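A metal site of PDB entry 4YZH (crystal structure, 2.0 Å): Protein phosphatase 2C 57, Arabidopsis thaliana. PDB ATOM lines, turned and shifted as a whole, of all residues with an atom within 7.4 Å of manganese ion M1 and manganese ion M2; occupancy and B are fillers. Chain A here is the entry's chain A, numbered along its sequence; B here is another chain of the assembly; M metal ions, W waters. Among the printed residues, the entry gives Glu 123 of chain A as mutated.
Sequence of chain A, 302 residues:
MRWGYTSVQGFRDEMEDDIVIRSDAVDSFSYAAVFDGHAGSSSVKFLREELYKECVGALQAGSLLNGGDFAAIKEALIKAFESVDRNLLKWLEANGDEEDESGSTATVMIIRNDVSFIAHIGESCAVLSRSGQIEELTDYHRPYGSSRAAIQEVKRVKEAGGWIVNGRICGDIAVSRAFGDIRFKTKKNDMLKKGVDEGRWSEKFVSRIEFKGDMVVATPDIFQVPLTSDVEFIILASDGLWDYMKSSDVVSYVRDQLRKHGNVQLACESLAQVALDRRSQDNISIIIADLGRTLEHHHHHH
Manganese ion M1 is bound by the side-chain carboxylate (OD2) of Asp 282, the side-chain carboxylate (OD1) of Asp 239, the side-chain carboxylate (OD2) of Asp 36, water W3, water W5 and water W2.
Water W2 lies within hydrogen-bond range of the side-chain carboxylate of Asp 17 (2.7 Å), the backbone carbonyl oxygen of Asn 283 (2.7 Å) and the side-chain hydroxyl of Ser 238 (3.2 Å). Water W3 lies within hydrogen-bond range of OD2 of Asp 239 (2.5 Å), O2P of TPO 3 of chain B (3.2 Å) and OE2 of Glu 123 (3.5 Å). Water W4 lies within hydrogen-bond range of OD1 of Asn 283 and OD1 of Asp 17. Water W1 lies within hydrogen-bond range of OE1 of Glu 16 (2.5 Å), NH1 of Arg 12 (3.3 Å) and O3P of TPO 3 of chain B (3.4 Å).
Within 4 Å of manganese ion M2: Asp 36, Gly 37 and TPO 3 of chain B. Along chain A the residues within 4 Å of manganese ion M2 span positions 36 to 37. The nearest printed residue that does not touch manganese ion M2 is Asp 17 (4.3 Å).
Of the 27 residues printed, 4 come within 4 Å of manganese ion M1. The nearest printed residue that does not touch manganese ion M1 is Asp 17 (4.4 Å).
O1P of TPO 3 of chain B is bound to manganese ion M2, at 2.1 Å. Manganese ion M2 is bound by OD1 of Asp 36 (2.2 Å). Water W1 binds manganese ion M2, at 2.4 Å. Water W5 binds manganese ion M2, 2.4 Å away. Manganese ion M2 is bound by O of Gly 37 (2.4 Å). Water W4 is bound to manganese ion M2 (2.5 Å). Manganese ion M2 has six donor atoms within binding distance.
The side-chain carboxylate of Asp 282 is in salt-bridge range of the guanidinium group of Arg 12. The backbone NH (N) of Thr 105 lies within hydrogen-bond range of the backbone carbonyl oxygen (O) of Asp 36, 3.0 Å away. O2P of TPO 3 of chain B lies within salt-bridge range of NH2 of Arg 12, at 2.5 Å. N of Gly 37 sits at hydrogen-bond distance from O of Glu 16, at 3.0 Å.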
ATOM      1  N   ARG A  12      -1.363  18.244   9.419  1.00  0.00           N
ATOM      2  CA  ARG A  12      -0.144  19.047   9.551  1.00  0.00           C
ATOM      3  C   ARG A  12       0.382  19.058  10.987  1.00  0.00           C
ATOM      4  O   ARG A  12      -0.378  18.918  11.931  1.00  0.00           O
ATOM      5  CB  ARG A  12      -0.415  20.480   9.097  1.00  0.00           C
ATOM      6  CG  ARG A  12      -0.604  20.625   7.597  1.00  0.00           C
ATOM      7  CD  ARG A  12       0.740  20.595   6.872  1.00  0.00           C
ATOM      8  NE  ARG A  12       0.603  21.046   5.500  1.00  0.00           N
ATOM      9  CZ  ARG A  12       1.024  22.220   5.046  1.00  0.00           C
ATOM     10  NH1 ARG A  12       1.649  23.055   5.843  1.00  0.00           N
ATOM     11  NH2 ARG A  12       0.841  22.534   3.779  1.00  0.00           N
ATOM     12  N   GLU A  14       1.551  21.668  12.427  1.00  0.00           N
ATOM     13  CA  GLU A  14       1.293  22.974  13.023  1.00  0.00           C
ATOM     14  C   GLU A  14      -0.001  23.559  12.446  1.00  0.00           C
ATOM     15  O   GLU A  14      -0.447  23.154  11.370  1.00  0.00           O
ATOM     16  CB  GLU A  14       2.462  23.933  12.763  1.00  0.00           C
ATOM     17  CG  GLU A  14       2.671  24.302  11.273  1.00  0.00           C
ATOM     18  CD  GLU A  14       3.274  23.171  10.439  1.00  0.00           C
ATOM     19  OE1 GLU A  14       4.329  22.619  10.832  1.00  0.00           O
ATOM     20  OE2 GLU A  14       2.699  22.833   9.386  1.00  0.00           O
ATOM     21  N   MET A  15      -0.623  24.486  13.180  1.00  0.00           N
ATOM     22  CA  MET A  15      -1.823  25.141  12.689  1.00  0.00           C
ATOM     23  C   MET A  15      -1.452  26.568  12.313  1.00  0.00           C
ATOM     24  O   MET A  15      -1.030  27.355  13.172  1.00  0.00           O
ATOM     25  CB  MET A  15      -2.917  25.149  13.759  1.00  0.00           C
ATOM     26  CG  MET A  15      -4.162  25.949  13.338  1.00  0.00           C
ATOM     27  SD  MET A  15      -4.816  25.344  11.768  1.00  0.00           S
ATOM     28  CE  MET A  15      -6.444  26.101  11.798  1.00  0.00           C
ATOM     29  N   GLU A  16      -1.595  26.899  11.034  1.00  0.00           N
ATOM     30  CA  GLU A  16      -1.240  28.240  10.553  1.00  0.00           C
ATOM     31  C   GLU A  16      -2.378  28.952   9.786  1.00  0.00           C
ATOM     32  O   GLU A  16      -2.175  30.078   9.344  1.00  0.00           O
ATOM     33  CB  GLU A  16       0.063  28.202   9.745  1.00  0.00           C
ATOM     34  CG  GLU A  16       1.300  27.791  10.605  1.00  0.00           C
ATOM     35  CD  GLU A  16       2.559  27.559   9.784  1.00  0.00           C
ATOM     36  OE1 GLU A  16       2.478  27.329   8.559  1.00  0.00           O
ATOM     37  OE2 GLU A  16       3.651  27.619  10.390  1.00  0.00           O
ATOM     38  N   ASP A  17      -3.547  28.319   9.666  1.00  0.00           N
ATOM     39  CA  ASP A  17      -4.756  29.005   9.104  1.00  0.00           C
ATOM     40  C   ASP A  17      -5.391  29.813  10.224  1.00  0.00           C
ATOM     41  O   ASP A  17      -5.217  29.502  11.396  1.00  0.00           O
ATOM     42  CB  ASP A  17      -5.835  28.010   8.663  1.00  0.00           C
ATOM     43  CG  ASP A  17      -5.658  27.428   7.245  1.00  0.00           C
ATOM     44  OD1 ASP A  17      -4.605  27.625   6.581  1.00  0.00           O
ATOM     45  OD2 ASP A  17      -6.612  26.708   6.803  1.00  0.00           O
ATOM     46  N   PHE A  35      -7.163  33.407   6.404  1.00  0.00           N
ATOM     47  CA  PHE A  35      -5.736  33.636   6.268  1.00  0.00           C
ATOM     48  C   PHE A  35      -5.035  32.299   6.287  1.00  0.00           C
ATOM     49  O   PHE A  35      -5.316  31.473   7.155  1.00  0.00           O
ATOM     50  CB  PHE A  35      -5.211  34.455   7.448  1.00  0.00           C
ATOM     51  CG  PHE A  35      -5.814  35.817   7.545  1.00  0.00           C
ATOM     52  CD1 PHE A  35      -5.573  36.749   6.544  1.00  0.00           C
ATOM     53  CD2 PHE A  35      -6.622  36.160   8.595  1.00  0.00           C
ATOM     54  CE1 PHE A  35      -6.148  38.014   6.605  1.00  0.00           C
ATOM     55  CE2 PHE A  35      -7.201  37.444   8.670  1.00  0.00           C
ATOM     56  CZ  PHE A  35      -6.952  38.366   7.665  1.00  0.00           C
ATOM     57  N   ASP A  36      -4.128  32.102   5.335  1.00  0.00           N
ATOM     58  CA  ASP A  36      -3.363  30.871   5.266  1.00  0.00           C
ATOM     59  C   ASP A  36      -1.895  31.236   5.446  1.00  0.00           C
ATOM     60  O   ASP A  36      -1.216  31.609   4.491  1.00  0.00           O
ATOM     61  CB  ASP A  36      -3.594  30.179   3.911  1.00  0.00           C
ATOM     62  CG  ASP A  36      -3.029  28.786   3.865  1.00  0.00           C
ATOM     63  OD1 ASP A  36      -2.065  28.550   4.570  1.00  0.00           O
ATOM     64  OD2 ASP A  36      -3.506  27.965   3.095  1.00  0.00           O
ATOM     65  N   GLY A  37      -1.422  31.149   6.685  1.00  0.00           N
ATOM     66  CA  GLY A  37      -0.021  31.456   6.969  1.00  0.00           C
ATOM     67  C   GLY A  37       0.961  30.367   6.607  1.00  0.00           C
ATOM     68  O   GLY A  37       0.606  29.214   6.455  1.00  0.00           O
ATOM     69  N   HIS A  38       2.225  30.738   6.456  1.00  0.00           N
ATOM     70  CA  HIS A  38       3.270  29.767   6.162  1.00  0.00           C
ATOM     71  C   HIS A  38       4.563  30.219   6.841  1.00  0.00           C
ATOM     72  O   HIS A  38       4.773  31.411   7.075  1.00  0.00           O
ATOM     73  CB  HIS A  38       3.496  29.623   4.655  1.00  0.00           C
ATOM     74  CG  HIS A  38       3.500  30.930   3.906  1.00  0.00           C
ATOM     75  ND1 HIS A  38       2.383  31.427   3.264  1.00  0.00           N
ATOM     76  CD2 HIS A  38       4.486  31.833   3.697  1.00  0.00           C
ATOM     77  CE1 HIS A  38       2.681  32.592   2.703  1.00  0.00           C
ATOM     78  NE2 HIS A  38       3.952  32.864   2.952  1.00  0.00           N
ATOM     79  N   ALA A  39       5.392  29.235   7.186  1.00  0.00           N
ATOM     80  CA  ALA A  39       6.668  29.469   7.873  1.00  0.00           C
ATOM     81  C   ALA A  39       6.499  30.244   9.163  1.00  0.00           C
ATOM     82  O   ALA A  39       7.272  31.173   9.434  1.00  0.00           O
ATOM     83  CB  ALA A  39       7.675  30.193   6.946  1.00  0.00           C
ATOM     84  N   GLY A  40       5.489  29.887   9.956  1.00  0.00           N
ATOM     85  CA  GLY A  40       5.244  30.550  11.226  1.00  0.00           C
ATOM     86  C   GLY A  40       3.854  31.165  11.282  1.00  0.00           C
ATOM     87  O   GLY A  40       3.122  31.162  10.290  1.00  0.00           O
ATOM     88  N   VAL A  44       0.097  35.946  10.204  1.00  0.00           N
ATOM     89  CA  VAL A  44      -1.335  35.724  10.402  1.00  0.00           C
ATOM     90  C   VAL A  44      -1.826  36.495  11.621  1.00  0.00           C
ATOM     91  O   VAL A  44      -2.877  37.134  11.589  1.00  0.00           O
ATOM     92  CB  VAL A  44      -1.674  34.230  10.610  1.00  0.00           C
ATOM     93  CG1 VAL A  44      -3.143  34.074  11.000  1.00  0.00           C
ATOM     94  CG2 VAL A  44      -1.410  33.464   9.370  1.00  0.00           C
ATOM     95  N   GLY A 103       4.901  34.412   6.540  1.00  0.00           N
ATOM     96  CA  GLY A 103       4.062  35.151   5.621  1.00  0.00           C
ATOM     97  C   GLY A 103       2.661  34.591   5.706  1.00  0.00           C
ATOM     98  O   GLY A 103       2.390  33.603   6.427  1.00  0.00           O
ATOM     99  N   THR A 105      -1.232  34.270   3.207  1.00  0.00           N
ATOM    100  CA  THR A 105      -2.155  34.696   2.160  1.00  0.00           C
ATOM    101  C   THR A 105      -3.435  35.191   2.805  1.00  0.00           C
ATOM    102  O   THR A 105      -3.593  35.110   4.041  1.00  0.00           O
ATOM    103  CB  THR A 105      -2.495  33.551   1.192  1.00  0.00           C
ATOM    104  OG1 THR A 105      -3.156  32.500   1.900  1.00  0.00           O
ATOM    105  CG2 THR A 105      -1.241  33.004   0.553  1.00  0.00           C
ATOM    106  N   GLU A 123      -3.874  31.405  -2.512  1.00  0.00           N
ATOM    107  CA  GLU A 123      -4.521  30.214  -3.087  1.00  0.00           C
ATOM    108  C   GLU A 123      -5.704  29.631  -2.295  1.00  0.00           C
ATOM    109  O   GLU A 123      -6.131  28.513  -2.534  1.00  0.00           O
ATOM    110  CB  GLU A 123      -3.473  29.134  -3.435  1.00  0.00           C
ATOM    111  CG  GLU A 123      -2.596  28.759  -2.277  1.00  0.00           C
ATOM    112  CD  GLU A 123      -1.433  27.830  -2.624  1.00  0.00           C
ATOM    113  OE1 GLU A 123      -1.404  27.211  -3.730  1.00  0.00           O
ATOM    114  OE2 GLU A 123      -0.535  27.730  -1.777  1.00  0.00           O
ATOM    115  N   SER A 124      -6.255  30.387  -1.348  1.00  0.00           N
ATOM    116  CA  SER A 124      -7.584  30.063  -0.854  1.00  0.00           C
ATOM    117  C   SER A 124      -8.532  30.414  -2.000  1.00  0.00           C
ATOM    118  O   SER A 124      -8.110  30.964  -3.012  1.00  0.00           O
ATOM    119  CB  SER A 124      -7.956  30.883   0.412  1.00  0.00           C
ATOM    120  OG  SER A 124      -7.146  30.492   1.523  1.00  0.00           O
ATOM    121  N   SER A 238      -9.743  27.670   2.846  1.00  0.00           N
ATOM    122  CA  SER A 238      -8.352  27.498   2.474  1.00  0.00           C
ATOM    123  C   SER A 238      -8.183  26.314   1.490  1.00  0.00           C
ATOM    124  O   SER A 238      -9.092  25.498   1.304  1.00  0.00           O
ATOM    125  CB  SER A 238      -7.464  27.293   3.705  1.00  0.00           C
ATOM    126  OG  SER A 238      -7.899  26.153   4.427  1.00  0.00           O
ATOM    127  N   ASP A 239      -7.011  26.228   0.891  1.00  0.00           N
ATOM    128  CA  ASP A 239      -6.755  25.189  -0.114  1.00  0.00           C
ATOM    129  C   ASP A 239      -6.727  23.782   0.522  1.00  0.00           C
ATOM    130  O   ASP A 239      -6.707  22.782  -0.199  1.00  0.00           O
ATOM    131  CB  ASP A 239      -5.474  25.479  -0.881  1.00  0.00           C
ATOM    132  CG  ASP A 239      -4.270  25.598   0.018  1.00  0.00           C
ATOM    133  OD1 ASP A 239      -4.461  25.531   1.245  1.00  0.00           O
ATOM    134  OD2 ASP A 239      -3.160  25.767  -0.510  1.00  0.00           O
ATOM    135  N   GLY A 240      -6.784  23.726   1.850  1.00  0.00           N
ATOM    136  CA  GLY A 240      -6.881  22.427   2.533  1.00  0.00           C
ATOM    137  C   GLY A 240      -8.186  21.740   2.154  1.00  0.00           C
ATOM    138  O   GLY A 240      -8.286  20.510   2.140  1.00  0.00           O
ATOM    139  N   LEU A 241      -9.186  22.555   1.835  1.00  0.00           N
ATOM    140  CA  LEU A 241     -10.443  22.000   1.297  1.00  0.00           C
ATOM    141  C   LEU A 241     -10.349  21.764  -0.226  1.00  0.00           C
ATOM    142  O   LEU A 241     -10.482  20.634  -0.699  1.00  0.00           O
ATOM    143  CB  LEU A 241     -11.629  22.939   1.597  1.00  0.00           C
ATOM    144  CG  LEU A 241     -12.959  22.555   0.914  1.00  0.00           C
ATOM    145  CD1 LEU A 241     -13.528  21.243   1.485  1.00  0.00           C
ATOM    146  CD2 LEU A 241     -14.030  23.679   0.963  1.00  0.00           C
ATOM    147  N   ASP A 243      -8.076  21.581  -2.558  1.00  0.00           N
ATOM    148  CA  ASP A 243      -7.111  20.658  -3.131  1.00  0.00           C
ATOM    149  C   ASP A 243      -7.626  19.219  -3.132  1.00  0.00           C
ATOM    150  O   ASP A 243      -7.134  18.396  -3.911  1.00  0.00           O
ATOM    151  CB  ASP A 243      -5.743  20.717  -2.392  1.00  0.00           C
ATOM    152  CG  ASP A 243      -4.932  21.989  -2.707  1.00  0.00           C
ATOM    153  OD1 ASP A 243      -5.333  22.760  -3.605  1.00  0.00           O
ATOM    154  OD2 ASP A 243      -3.886  22.220  -2.052  1.00  0.00           O
ATOM    155  N   ASP A 282      -3.520  19.254   4.675  1.00  0.00           N
ATOM    156  CA  ASP A 282      -3.270  20.617   5.087  1.00  0.00           C
ATOM    157  C   ASP A 282      -4.238  21.027   6.193  1.00  0.00           C
ATOM    158  O   ASP A 282      -5.237  20.337   6.440  1.00  0.00           O
ATOM    159  CB  ASP A 282      -3.503  21.516   3.879  1.00  0.00           C
ATOM    160  CG  ASP A 282      -2.843  22.874   4.016  1.00  0.00           C
ATOM    161  OD1 ASP A 282      -2.196  23.209   5.032  1.00  0.00           O
ATOM    162  OD2 ASP A 282      -2.971  23.583   3.042  1.00  0.00           O
ATOM    163  N   ASN A 283      -3.972  22.174   6.821  1.00  0.00           N
ATOM    164  CA  ASN A 283      -4.955  22.823   7.682  1.00  0.00           C
ATOM    165  C   ASN A 283      -6.156  23.127   6.782  1.00  0.00           C
ATOM    166  O   ASN A 283      -5.982  23.398   5.583  1.00  0.00           O
ATOM    167  CB  ASN A 283      -4.459  24.169   8.253  1.00  0.00           C
ATOM    168  CG  ASN A 283      -3.104  24.079   8.978  1.00  0.00           C
ATOM    169  OD1 ASN A 283      -2.323  25.047   8.932  1.00  0.00           O
ATOM    170  ND2 ASN A 283      -2.834  22.944   9.665  1.00  0.00           N
ATOM    171  N   ILE A 284      -7.347  23.076   7.349  1.00  0.00           N
ATOM    172  CA  ILE A 284      -8.604  23.259   6.613  1.00  0.00           C
ATOM    173  C   ILE A 284      -9.445  24.297   7.339  1.00  0.00           C
ATOM    174  O   ILE A 284      -9.792  24.103   8.494  1.00  0.00           O
ATOM    175  CB  ILE A 284      -9.388  21.923   6.574  1.00  0.00           C
ATOM    176  CG1 ILE A 284      -8.585  20.862   5.805  1.00  0.00           C
ATOM    177  CG2 ILE A 284     -10.803  22.131   5.977  1.00  0.00           C
ATOM    178  CD1 ILE A 284      -8.909  19.403   6.190  1.00  0.00           C
ATOM    179  N   ARG B   1       0.646  20.897  -0.248  1.00  0.00           N
ATOM    180  CA  ARG B   1       2.089  20.850  -0.136  1.00  0.00           C
ATOM    181  C   ARG B   1       2.621  21.951   0.782  1.00  0.00           C
ATOM    182  O   ARG B   1       2.018  22.998   0.903  1.00  0.00           O
ATOM    183  CB  ARG B   1       2.728  20.981  -1.519  1.00  0.00           C
ATOM    184  CG  ARG B   1       2.807  22.413  -2.026  1.00  0.00           C
ATOM    185  CD  ARG B   1       2.621  22.489  -3.535  1.00  0.00           C
ATOM    186  NE  ARG B   1       3.893  22.430  -4.236  1.00  0.00           N
ATOM    187  CZ  ARG B   1       4.031  22.120  -5.510  1.00  0.00           C
ATOM    188  NH1 ARG B   1       2.951  21.856  -6.249  1.00  0.00           N
ATOM    189  NH2 ARG B   1       5.231  22.088  -6.069  1.00  0.00           N
ATOM    190  N   LYS B   2       3.751  21.691   1.431  1.00  0.00           N
ATOM    191  CA  LYS B   2       4.400  22.716   2.232  1.00  0.00           C
ATOM    192  C   LYS B   2       4.611  23.945   1.360  1.00  0.00           C
ATOM    193  O   LYS B   2       5.082  23.842   0.243  1.00  0.00           O
ATOM    194  CB  LYS B   2       5.730  22.212   2.775  1.00  0.00           C
ATOM    195  CG  LYS B   2       6.416  23.183   3.713  1.00  0.00           C
ATOM    196  CD  LYS B   2       7.318  22.458   4.701  1.00  0.00           C
ATOM    197  CE  LYS B   2       8.083  23.425   5.572  1.00  0.00           C
ATOM    198  NZ  LYS B   2       9.261  22.790   6.229  1.00  0.00           N
ATOM    199  N   TPO B   3       4.213  25.108   1.863  1.00  0.00           N
ATOM    200  CA  TPO B   3       4.166  26.316   1.044  1.00  0.00           C
ATOM    201  CB  TPO B   3       3.226  27.319   1.704  1.00  0.00           C
ATOM    202  CG2 TPO B   3       2.971  28.523   0.808  1.00  0.00           C
ATOM    203  OG1 TPO B   3       1.980  26.687   1.972  1.00  0.00           O
ATOM    204  P   TPO B   3       1.639  26.255   3.471  1.00  0.00           P
ATOM    205  O1P TPO B   3       0.936  27.440   4.038  1.00  0.00           O
ATOM    206  O2P TPO B   3       0.772  25.039   3.344  1.00  0.00           O
ATOM    207  O3P TPO B   3       2.985  25.997   4.100  1.00  0.00           O
ATOM    208  C   TPO B   3       5.511  26.932   0.780  1.00  0.00           C
ATOM    209  O   TPO B   3       5.650  27.742  -0.145  1.00  0.00           O
HETATM  210 MN    MN M   1      -3.007  25.791   2.913  1.00  0.00          MN
HETATM  211 MN    MN M   2      -0.497  27.291   5.501  1.00  0.00          MN
HETATM  212  O   HOH W   1       1.002  26.135   6.915  1.00  0.00           O
HETATM  213  O   HOH W   2      -4.760  25.678   4.658  1.00  0.00           O
HETATM  214  O   HOH W   3      -1.401  26.190   1.227  1.00  0.00           O
HETATM  215  O   HOH W   4      -2.184  27.135   7.391  1.00  0.00           O
HETATM  216  O   HOH W   5      -1.195  25.318   4.399  1.00  0.00           O
